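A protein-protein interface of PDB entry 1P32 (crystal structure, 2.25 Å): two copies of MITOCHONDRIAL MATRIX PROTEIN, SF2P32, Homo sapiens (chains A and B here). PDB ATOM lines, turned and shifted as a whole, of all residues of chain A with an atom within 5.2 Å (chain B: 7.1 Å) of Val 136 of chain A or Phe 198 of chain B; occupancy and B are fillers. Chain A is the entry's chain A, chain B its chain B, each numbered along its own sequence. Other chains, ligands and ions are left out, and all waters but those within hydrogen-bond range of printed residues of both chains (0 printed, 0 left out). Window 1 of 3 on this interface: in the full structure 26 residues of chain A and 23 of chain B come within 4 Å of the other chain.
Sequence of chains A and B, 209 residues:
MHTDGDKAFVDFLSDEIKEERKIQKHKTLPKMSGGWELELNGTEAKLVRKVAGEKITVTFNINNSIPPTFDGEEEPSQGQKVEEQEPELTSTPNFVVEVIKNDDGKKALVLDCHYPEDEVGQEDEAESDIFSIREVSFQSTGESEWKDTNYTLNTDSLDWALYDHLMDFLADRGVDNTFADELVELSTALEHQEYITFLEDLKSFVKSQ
Val 136 of chain A touches Phe 198 of chain B (CG1 to CZ, 3.9 Å).
CE1 of Phe 198 of chain B touches CD2 of Phe 138 of chain A, at 3.6 Å.
Phe 138 of chain A touches Asp 201 of chain B (CZ to O, 3.6 Å).
Phe 138 of chain A touches Leu 202 of chain B.
CD1 of Tyr 151 of chain A touches CB of Glu 194 of chain B, 3.7 Å away.
OH of Tyr 151 of chain A touches CD1 of Tyr 195 of chain B (3.6 Å).
CD2 of Tyr 151 of chain A touches CG of Phe 198 of chain B, at 3.5 Å.
CE1 of Tyr 195 of chain B touches CD1 of Leu 153 of chain A, 3.7 Å away.
Phe 198 of chain B touches Leu 153 of chain A (CE2 to CD2, 3.7 Å).
The backbone carbonyl oxygen (O) of Val 136 of chain A sits at hydrogen-bond distance from the backbone NH (N) of Leu 153 of chain A (2.8 Å).
No position is printed for both chains.
Val 136 of chain A touches one residue of chain B.
Printed residues of chain B within 4 Å of Leu 153 of chain A: Tyr 195 and Phe 198.
Of the printed residues of chain A, Tyr 195 of chain B touches Tyr 151 and Leu 153.
Phe 198 of chain B touches just these residues of chain A: Val 136, Phe 138, Tyr 151 and Leu 153.
The nearest residue of chain B that does not touch Val 136 of chain A is Leu 202 of chain B (5.4 Å).
The nearest residue of chain A that does not touch Phe 198 of chain B is Ser 137 of chain A (4.1 Å).
Printed residues of chain B that touch a printed residue of chain A: Glu 194, Tyr 195, Phe 198, Asp 201 and Leu 202.
Hydrophobic or aromatic side chains of chain B that line the printed part of chain A: Tyr 195 and Phe 198.
Along chain B the printed residues that touch a printed residue of chain A span positions 194 to 202.
Among the printed residues, no Asp or Glu carboxylate lies within 4 Å of a Lys or Arg side-chain nitrogen of the other chain.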
ATOM      1  N   LEU A 109      20.319 -12.216  -4.416  1.00  0.00           N
ATOM      2  CA  LEU A 109      19.481 -11.241  -3.734  1.00  0.00           C
ATOM      3  C   LEU A 109      18.730 -12.087  -2.693  1.00  0.00           C
ATOM      4  O   LEU A 109      18.077 -13.073  -3.040  1.00  0.00           O
ATOM      5  CB  LEU A 109      18.501 -10.590  -4.723  1.00  0.00           C
ATOM      6  CG  LEU A 109      17.505  -9.586  -4.120  1.00  0.00           C
ATOM      7  CD1 LEU A 109      18.261  -8.435  -3.508  1.00  0.00           C
ATOM      8  CD2 LEU A 109      16.548  -9.085  -5.185  1.00  0.00           C
ATOM      9  N   VAL A 110      18.841 -11.711  -1.425  1.00  0.00           N
ATOM     10  CA  VAL A 110      18.213 -12.459  -0.339  1.00  0.00           C
ATOM     11  C   VAL A 110      17.109 -11.673   0.367  1.00  0.00           C
ATOM     12  O   VAL A 110      17.332 -10.564   0.853  1.00  0.00           O
ATOM     13  CB  VAL A 110      19.291 -12.886   0.699  1.00  0.00           C
ATOM     14  CG1 VAL A 110      18.667 -13.720   1.806  1.00  0.00           C
ATOM     15  CG2 VAL A 110      20.397 -13.679  -0.001  1.00  0.00           C
ATOM     16  N   LEU A 111      15.913 -12.251   0.419  1.00  0.00           N
ATOM     17  CA  LEU A 111      14.793 -11.590   1.067  1.00  0.00           C
ATOM     18  C   LEU A 111      14.230 -12.401   2.233  1.00  0.00           C
ATOM     19  O   LEU A 111      13.658 -13.480   2.048  1.00  0.00           O
ATOM     20  CB  LEU A 111      13.691 -11.290   0.046  1.00  0.00           C
ATOM     21  CG  LEU A 111      14.147 -10.555  -1.221  1.00  0.00           C
ATOM     22  CD1 LEU A 111      14.639 -11.579  -2.256  1.00  0.00           C
ATOM     23  CD2 LEU A 111      12.997  -9.762  -1.804  1.00  0.00           C
ATOM     24  N   ASP A 112      14.401 -11.863   3.437  1.00  0.00           N
ATOM     25  CA  ASP A 112      13.926 -12.489   4.666  1.00  0.00           C
ATOM     26  C   ASP A 112      12.449 -12.134   4.824  1.00  0.00           C
ATOM     27  O   ASP A 112      12.094 -10.966   4.969  1.00  0.00           O
ATOM     28  CB  ASP A 112      14.722 -11.948   5.859  1.00  0.00           C
ATOM     29  CG  ASP A 112      14.347 -12.620   7.178  1.00  0.00           C
ATOM     30  OD1 ASP A 112      14.768 -12.111   8.239  1.00  0.00           O
ATOM     31  OD2 ASP A 112      13.650 -13.659   7.160  1.00  0.00           O
ATOM     32  N   ILE A 133       7.910  -8.835   3.688  1.00  0.00           N
ATOM     33  CA  ILE A 133       9.359  -8.864   3.556  1.00  0.00           C
ATOM     34  C   ILE A 133       9.879  -8.007   4.696  1.00  0.00           C
ATOM     35  O   ILE A 133       9.415  -6.882   4.878  1.00  0.00           O
ATOM     36  CB  ILE A 133       9.804  -8.239   2.224  1.00  0.00           C
ATOM     37  CG1 ILE A 133       9.184  -9.003   1.051  1.00  0.00           C
ATOM     38  CG2 ILE A 133      11.321  -8.263   2.119  1.00  0.00           C
ATOM     39  CD1 ILE A 133       9.416  -8.333  -0.291  1.00  0.00           C
ATOM     40  N   ARG A 134      10.829  -8.532   5.466  1.00  0.00           N
ATOM     41  CA  ARG A 134      11.393  -7.781   6.589  1.00  0.00           C
ATOM     42  C   ARG A 134      12.776  -7.212   6.311  1.00  0.00           C
ATOM     43  O   ARG A 134      13.119  -6.137   6.807  1.00  0.00           O
ATOM     44  CB  ARG A 134      11.430  -8.655   7.846  1.00  0.00           C
ATOM     45  CG  ARG A 134      10.043  -9.076   8.297  1.00  0.00           C
ATOM     46  CD  ARG A 134       9.154  -7.847   8.497  1.00  0.00           C
ATOM     47  NE  ARG A 134       7.757  -8.188   8.744  1.00  0.00           N
ATOM     48  CZ  ARG A 134       6.788  -7.296   8.923  1.00  0.00           C
ATOM     49  NH1 ARG A 134       7.059  -5.999   8.882  1.00  0.00           N
ATOM     50  NH2 ARG A 134       5.543  -7.700   9.139  1.00  0.00           N
ATOM     51  N   GLU A 135      13.564  -7.927   5.510  1.00  0.00           N
ATOM     52  CA  GLU A 135      14.910  -7.488   5.171  1.00  0.00           C
ATOM     53  C   GLU A 135      15.328  -7.965   3.796  1.00  0.00           C
ATOM     54  O   GLU A 135      14.941  -9.044   3.357  1.00  0.00           O
ATOM     55  CB  GLU A 135      15.938  -8.005   6.187  1.00  0.00           C
ATOM     56  CG  GLU A 135      15.721  -7.539   7.601  1.00  0.00           C
ATOM     57  CD  GLU A 135      16.918  -7.832   8.477  1.00  0.00           C
ATOM     58  OE1 GLU A 135      17.350  -9.004   8.522  1.00  0.00           O
ATOM     59  OE2 GLU A 135      17.425  -6.890   9.124  1.00  0.00           O
ATOM     60  N   VAL A 136      16.134  -7.151   3.125  1.00  0.00           N
ATOM     61  CA  VAL A 136      16.630  -7.491   1.803  1.00  0.00           C
ATOM     62  C   VAL A 136      18.112  -7.153   1.749  1.00  0.00           C
ATOM     63  O   VAL A 136      18.549  -6.160   2.327  1.00  0.00           O
ATOM     64  CB  VAL A 136      15.893  -6.695   0.697  1.00  0.00           C
ATOM     65  CG1 VAL A 136      16.427  -7.098  -0.677  1.00  0.00           C
ATOM     66  CG2 VAL A 136      14.410  -6.953   0.775  1.00  0.00           C
ATOM     67  N   SER A 137      18.886  -7.994   1.074  1.00  0.00           N
ATOM     68  CA  SER A 137      20.313  -7.755   0.943  1.00  0.00           C
ATOM     69  C   SER A 137      20.923  -8.670  -0.104  1.00  0.00           C
ATOM     70  O   SER A 137      20.282  -9.604  -0.584  1.00  0.00           O
ATOM     71  CB  SER A 137      21.020  -8.003   2.273  1.00  0.00           C
ATOM     72  OG  SER A 137      20.949  -9.371   2.630  1.00  0.00           O
ATOM     73  N   PHE A 138      22.168  -8.381  -0.457  1.00  0.00           N
ATOM     74  CA  PHE A 138      22.921  -9.192  -1.398  1.00  0.00           C
ATOM     75  C   PHE A 138      23.897 -10.007  -0.555  1.00  0.00           C
ATOM     76  O   PHE A 138      24.542  -9.472   0.345  1.00  0.00           O
ATOM     77  CB  PHE A 138      23.694  -8.303  -2.378  1.00  0.00           C
ATOM     78  CG  PHE A 138      22.847  -7.729  -3.474  1.00  0.00           C
ATOM     79  CD1 PHE A 138      22.430  -8.528  -4.535  1.00  0.00           C
ATOM     80  CD2 PHE A 138      22.439  -6.402  -3.434  1.00  0.00           C
ATOM     81  CE1 PHE A 138      21.622  -8.015  -5.536  1.00  0.00           C
ATOM     82  CE2 PHE A 138      21.626  -5.880  -4.433  1.00  0.00           C
ATOM     83  CZ  PHE A 138      21.217  -6.688  -5.485  1.00  0.00           C
ATOM     84  N   TYR A 151      25.346  -4.705   3.278  1.00  0.00           N
ATOM     85  CA  TYR A 151      24.204  -3.833   3.506  1.00  0.00           C
ATOM     86  C   TYR A 151      22.899  -4.620   3.558  1.00  0.00           C
ATOM     87  O   TYR A 151      22.608  -5.422   2.672  1.00  0.00           O
ATOM     88  CB  TYR A 151      24.093  -2.772   2.412  1.00  0.00           C
ATOM     89  CG  TYR A 151      22.978  -1.779   2.671  1.00  0.00           C
ATOM     90  CD1 TYR A 151      23.123  -0.761   3.623  1.00  0.00           C
ATOM     91  CD2 TYR A 151      21.753  -1.896   2.016  1.00  0.00           C
ATOM     92  CE1 TYR A 151      22.070   0.112   3.914  1.00  0.00           C
ATOM     93  CE2 TYR A 151      20.696  -1.032   2.300  1.00  0.00           C
ATOM     94  CZ  TYR A 151      20.860  -0.035   3.248  1.00  0.00           C
ATOM     95  OH  TYR A 151      19.809   0.804   3.527  1.00  0.00           O
ATOM     96  N   THR A 152      22.118  -4.371   4.603  1.00  0.00           N
ATOM     97  CA  THR A 152      20.830  -5.027   4.796  1.00  0.00           C
ATOM     98  C   THR A 152      19.759  -3.957   4.951  1.00  0.00           C
ATOM     99  O   THR A 152      19.804  -3.147   5.874  1.00  0.00           O
ATOM    100  CB  THR A 152      20.845  -5.917   6.048  1.00  0.00           C
ATOM    101  OG1 THR A 152      21.815  -6.957   5.873  1.00  0.00           O
ATOM    102  CG2 THR A 152      19.471  -6.537   6.287  1.00  0.00           C
ATOM    103  N   LEU A 153      18.805  -3.961   4.029  1.00  0.00           N
ATOM    104  CA  LEU A 153      17.715  -2.997   4.018  1.00  0.00           C
ATOM    105  C   LEU A 153      16.520  -3.462   4.847  1.00  0.00           C
ATOM    106  O   LEU A 153      15.875  -4.457   4.519  1.00  0.00           O
ATOM    107  CB  LEU A 153      17.263  -2.764   2.577  1.00  0.00           C
ATOM    108  CG  LEU A 153      16.114  -1.788   2.337  1.00  0.00           C
ATOM    109  CD1 LEU A 153      16.540  -0.377   2.718  1.00  0.00           C
ATOM    110  CD2 LEU A 153      15.720  -1.843   0.873  1.00  0.00           C
ATOM    111  N   THR A 155      12.778  -3.174   5.997  1.00  0.00           N
ATOM    112  CA  THR A 155      11.574  -2.665   5.336  1.00  0.00           C
ATOM    113  C   THR A 155      10.629  -1.822   6.195  1.00  0.00           C
ATOM    114  O   THR A 155       9.647  -1.299   5.681  1.00  0.00           O
ATOM    115  CB  THR A 155      10.735  -3.812   4.730  1.00  0.00           C
ATOM    116  OG1 THR A 155      10.257  -4.654   5.784  1.00  0.00           O
ATOM    117  CG2 THR A 155      11.570  -4.645   3.773  1.00  0.00           C
ATOM    118  N   LEU A 166       9.181  -4.921  -4.810  1.00  0.00           N
ATOM    119  CA  LEU A 166       9.863  -6.097  -4.281  1.00  0.00           C
ATOM    120  C   LEU A 166       8.870  -7.250  -4.240  1.00  0.00           C
ATOM    121  O   LEU A 166       9.201  -8.387  -4.600  1.00  0.00           O
ATOM    122  CB  LEU A 166      10.409  -5.817  -2.876  1.00  0.00           C
ATOM    123  CG  LEU A 166      11.628  -4.884  -2.872  1.00  0.00           C
ATOM    124  CD1 LEU A 166      11.949  -4.363  -1.465  1.00  0.00           C
ATOM    125  CD2 LEU A 166      12.799  -5.658  -3.452  1.00  0.00           C
ATOM    126  N   LEU B  13      13.541   2.548 -10.019  1.00  0.00           N
ATOM    127  CA  LEU B  13      14.824   2.704  -9.347  1.00  0.00           C
ATOM    128  C   LEU B  13      15.650   3.852  -9.946  1.00  0.00           C
ATOM    129  O   LEU B  13      16.311   4.593  -9.214  1.00  0.00           O
ATOM    130  CB  LEU B  13      15.604   1.382  -9.388  1.00  0.00           C
ATOM    131  CG  LEU B  13      15.011   0.250  -8.530  1.00  0.00           C
ATOM    132  CD1 LEU B  13      15.721  -1.062  -8.804  1.00  0.00           C
ATOM    133  CD2 LEU B  13      15.128   0.614  -7.062  1.00  0.00           C
ATOM    134  N   ILE B  17      16.783   6.798  -7.454  1.00  0.00           N
ATOM    135  CA  ILE B  17      18.213   7.057  -7.314  1.00  0.00           C
ATOM    136  C   ILE B  17      18.514   8.520  -7.653  1.00  0.00           C
ATOM    137  O   ILE B  17      19.314   9.171  -6.985  1.00  0.00           O
ATOM    138  CB  ILE B  17      19.031   6.137  -8.245  1.00  0.00           C
ATOM    139  CG1 ILE B  17      18.883   4.682  -7.784  1.00  0.00           C
ATOM    140  CG2 ILE B  17      20.495   6.566  -8.270  1.00  0.00           C
ATOM    141  CD1 ILE B  17      19.537   3.672  -8.707  1.00  0.00           C
ATOM    142  N   HIS B 192      22.594   6.458   4.607  1.00  0.00           N
ATOM    143  CA  HIS B 192      21.970   6.986   3.400  1.00  0.00           C
ATOM    144  C   HIS B 192      22.799   6.760   2.142  1.00  0.00           C
ATOM    145  O   HIS B 192      22.249   6.550   1.063  1.00  0.00           O
ATOM    146  CB  HIS B 192      21.659   8.472   3.574  1.00  0.00           C
ATOM    147  CG  HIS B 192      20.712   9.009   2.545  1.00  0.00           C
ATOM    148  ND1 HIS B 192      21.028   9.074   1.206  1.00  0.00           N
ATOM    149  CD2 HIS B 192      19.446   9.474   2.657  1.00  0.00           C
ATOM    150  CE1 HIS B 192      19.997   9.558   0.536  1.00  0.00           C
ATOM    151  NE2 HIS B 192      19.024   9.807   1.392  1.00  0.00           N
ATOM    152  N   GLN B 193      24.119   6.796   2.278  1.00  0.00           N
ATOM    153  CA  GLN B 193      24.991   6.572   1.136  1.00  0.00           C
ATOM    154  C   GLN B 193      25.028   5.097   0.764  1.00  0.00           C
ATOM    155  O   GLN B 193      25.118   4.751  -0.411  1.00  0.00           O
ATOM    156  CB  GLN B 193      26.412   7.054   1.431  1.00  0.00           C
ATOM    157  CG  GLN B 193      26.520   8.549   1.657  1.00  0.00           C
ATOM    158  CD  GLN B 193      27.955   9.012   1.837  1.00  0.00           C
ATOM    159  OE1 GLN B 193      28.215  10.199   2.050  1.00  0.00           O
ATOM    160  NE2 GLN B 193      28.896   8.074   1.751  1.00  0.00           N
ATOM    161  N   GLU B 194      24.963   4.220   1.760  1.00  0.00           N
ATOM    162  CA  GLU B 194      24.997   2.801   1.455  1.00  0.00           C
ATOM    163  C   GLU B 194      23.652   2.353   0.918  1.00  0.00           C
ATOM    164  O   GLU B 194      23.561   1.362   0.199  1.00  0.00           O
ATOM    165  CB  GLU B 194      25.415   1.997   2.685  1.00  0.00           C
ATOM    166  CG  GLU B 194      26.804   2.400   3.165  1.00  0.00           C
ATOM    167  CD  GLU B 194      27.458   1.371   4.061  1.00  0.00           C
ATOM    168  OE1 GLU B 194      28.535   1.677   4.613  1.00  0.00           O
ATOM    169  OE2 GLU B 194      26.912   0.258   4.202  1.00  0.00           O
ATOM    170  N   TYR B 195      22.613   3.106   1.255  1.00  0.00           N
ATOM    171  CA  TYR B 195      21.271   2.821   0.770  1.00  0.00           C
ATOM    172  C   TYR B 195      21.263   3.124  -0.726  1.00  0.00           C
ATOM    173  O   TYR B 195      20.727   2.363  -1.533  1.00  0.00           O
ATOM    174  CB  TYR B 195      20.257   3.722   1.475  1.00  0.00           C
ATOM    175  CG  TYR B 195      18.868   3.675   0.880  1.00  0.00           C
ATOM    176  CD1 TYR B 195      18.115   2.500   0.899  1.00  0.00           C
ATOM    177  CD2 TYR B 195      18.299   4.815   0.309  1.00  0.00           C
ATOM    178  CE1 TYR B 195      16.820   2.464   0.364  1.00  0.00           C
ATOM    179  CE2 TYR B 195      17.009   4.791  -0.227  1.00  0.00           C
ATOM    180  CZ  TYR B 195      16.275   3.613  -0.195  1.00  0.00           C
ATOM    181  OH  TYR B 195      14.999   3.588  -0.719  1.00  0.00           O
ATOM    182  N   ILE B 196      21.868   4.250  -1.090  1.00  0.00           N
ATOM    183  CA  ILE B 196      21.928   4.654  -2.484  1.00  0.00           C
ATOM    184  C   ILE B 196      22.732   3.633  -3.275  1.00  0.00           C
ATOM    185  O   ILE B 196      22.320   3.214  -4.354  1.00  0.00           O
ATOM    186  CB  ILE B 196      22.552   6.056  -2.619  1.00  0.00           C
ATOM    187  CG1 ILE B 196      21.664   7.074  -1.894  1.00  0.00           C
ATOM    188  CG2 ILE B 196      22.695   6.430  -4.089  1.00  0.00           C
ATOM    189  CD1 ILE B 196      22.263   8.468  -1.792  1.00  0.00           C
ATOM    190  N   THR B 197      23.871   3.223  -2.731  1.00  0.00           N
ATOM    191  CA  THR B 197      24.704   2.229  -3.391  1.00  0.00           C
ATOM    192  C   THR B 197      23.874   0.965  -3.583  1.00  0.00           C
ATOM    193  O   THR B 197      23.918   0.330  -4.634  1.00  0.00           O
ATOM    194  CB  THR B 197      25.937   1.882  -2.535  1.00  0.00           C
ATOM    195  OG1 THR B 197      26.755   3.049  -2.381  1.00  0.00           O
ATOM    196  CG2 THR B 197      26.748   0.779  -3.190  1.00  0.00           C
ATOM    197  N   PHE B 198      23.112   0.609  -2.557  1.00  0.00           N
ATOM    198  CA  PHE B 198      22.271  -0.570  -2.617  1.00  0.00           C
ATOM    199  C   PHE B 198      21.239  -0.478  -3.745  1.00  0.00           C
ATOM    200  O   PHE B 198      21.027  -1.443  -4.479  1.00  0.00           O
ATOM    201  CB  PHE B 198      21.538  -0.773  -1.292  1.00  0.00           C
ATOM    202  CG  PHE B 198      20.630  -1.970  -1.289  1.00  0.00           C
ATOM    203  CD1 PHE B 198      21.156  -3.258  -1.247  1.00  0.00           C
ATOM    204  CD2 PHE B 198      19.250  -1.812  -1.389  1.00  0.00           C
ATOM    205  CE1 PHE B 198      20.321  -4.378  -1.308  1.00  0.00           C
ATOM    206  CE2 PHE B 198      18.405  -2.924  -1.452  1.00  0.00           C
ATOM    207  CZ  PHE B 198      18.943  -4.207  -1.412  1.00  0.00           C
ATOM    208  N   LEU B 199      20.583   0.672  -3.872  1.00  0.00           N
ATOM    209  CA  LEU B 199      19.579   0.844  -4.920  1.00  0.00           C
ATOM    210  C   LEU B 199      20.196   0.625  -6.302  1.00  0.00           C
ATOM    211  O   LEU B 199      19.563   0.065  -7.201  1.00  0.00           O
ATOM    212  CB  LEU B 199      18.946   2.242  -4.847  1.00  0.00           C
ATOM    213  CG  LEU B 199      18.081   2.577  -3.624  1.00  0.00           C
ATOM    214  CD1 LEU B 199      17.578   4.029  -3.715  1.00  0.00           C
ATOM    215  CD2 LEU B 199      16.898   1.612  -3.564  1.00  0.00           C
ATOM    216  N   GLU B 200      21.436   1.074  -6.463  1.00  0.00           N
ATOM    217  CA  GLU B 200      22.154   0.919  -7.724  1.00  0.00           C
ATOM    218  C   GLU B 200      22.490  -0.546  -7.975  1.00  0.00           C
ATOM    219  O   GLU B 200      22.385  -1.026  -9.100  1.00  0.00           O
ATOM    220  CB  GLU B 200      23.429   1.771  -7.702  1.00  0.00           C
ATOM    221  CG  GLU B 200      23.131   3.260  -7.726  1.00  0.00           C
ATOM    222  CD  GLU B 200      24.354   4.126  -7.511  1.00  0.00           C
ATOM    223  OE1 GLU B 200      24.240   5.352  -7.718  1.00  0.00           O
ATOM    224  OE2 GLU B 200      25.418   3.592  -7.123  1.00  0.00           O
ATOM    225  N   ASP B 201      22.899  -1.256  -6.929  1.00  0.00           N
ATOM    226  CA  ASP B 201      23.212  -2.673  -7.063  1.00  0.00           C
ATOM    227  C   ASP B 201      21.947  -3.446  -7.411  1.00  0.00           C
ATOM    228  O   ASP B 201      21.986  -4.405  -8.185  1.00  0.00           O
ATOM    229  CB  ASP B 201      23.798  -3.218  -5.763  1.00  0.00           C
ATOM    230  CG  ASP B 201      25.197  -2.710  -5.499  1.00  0.00           C
ATOM    231  OD1 ASP B 201      25.718  -2.942  -4.388  1.00  0.00           O
ATOM    232  OD2 ASP B 201      25.779  -2.083  -6.409  1.00  0.00           O
ATOM    233  N   LEU B 202      20.830  -3.011  -6.834  1.00  0.00           N
ATOM    234  CA  LEU B 202      19.539  -3.648  -7.060  1.00  0.00           C
ATOM    235  C   LEU B 202      19.090  -3.424  -8.495  1.00  0.00           C
ATOM    236  O   LEU B 202      18.516  -4.315  -9.116  1.00  0.00           O
ATOM    237  CB  LEU B 202      18.492  -3.076  -6.094  1.00  0.00           C
ATOM    238  CG  LEU B 202      17.077  -3.666  -6.088  1.00  0.00           C
ATOM    239  CD1 LEU B 202      17.113  -5.159  -5.718  1.00  0.00           C
ATOM    240  CD2 LEU B 202      16.231  -2.894  -5.081  1.00  0.00           C
ATOM    241  N   LYS B 203      19.360  -2.230  -9.014  1.00  0.00           N
ATOM    242  CA  LYS B 203      18.981  -1.883 -10.379  1.00  0.00           C
ATOM    243  C   LYS B 203      19.742  -2.748 -11.374  1.00  0.00           C
ATOM    244  O   LYS B 203      19.155  -3.283 -12.315  1.00  0.00           O
ATOM    245  CB  LYS B 203      19.268  -0.402 -10.660  1.00  0.00           C
ATOM    246  CG  LYS B 203      18.951   0.029 -12.089  1.00  0.00           C
ATOM    247  CD  LYS B 203      19.339   1.483 -12.332  1.00  0.00           C
ATOM    248  CE  LYS B 203      19.168   1.865 -13.793  1.00  0.00           C
ATOM    249  NZ  LYS B 203      19.635   3.257 -14.065  1.00  0.00           N
ATOM    250  N   SER B 204      21.051  -2.877 -11.163  1.00  0.00           N
ATOM    251  CA  SER B 204      21.898  -3.689 -12.033  1.00  0.00           C
ATOM    252  C   SER B 204      21.475  -5.155 -11.994  1.00  0.00           C
ATOM    253  O   SER B 204      21.502  -5.844 -13.011  1.00  0.00           O
ATOM    254  CB  SER B 204      23.362  -3.585 -11.599  1.00  0.00           C
ATOM    255  OG  SER B 204      23.817  -2.245 -11.656  1.00  0.00           O
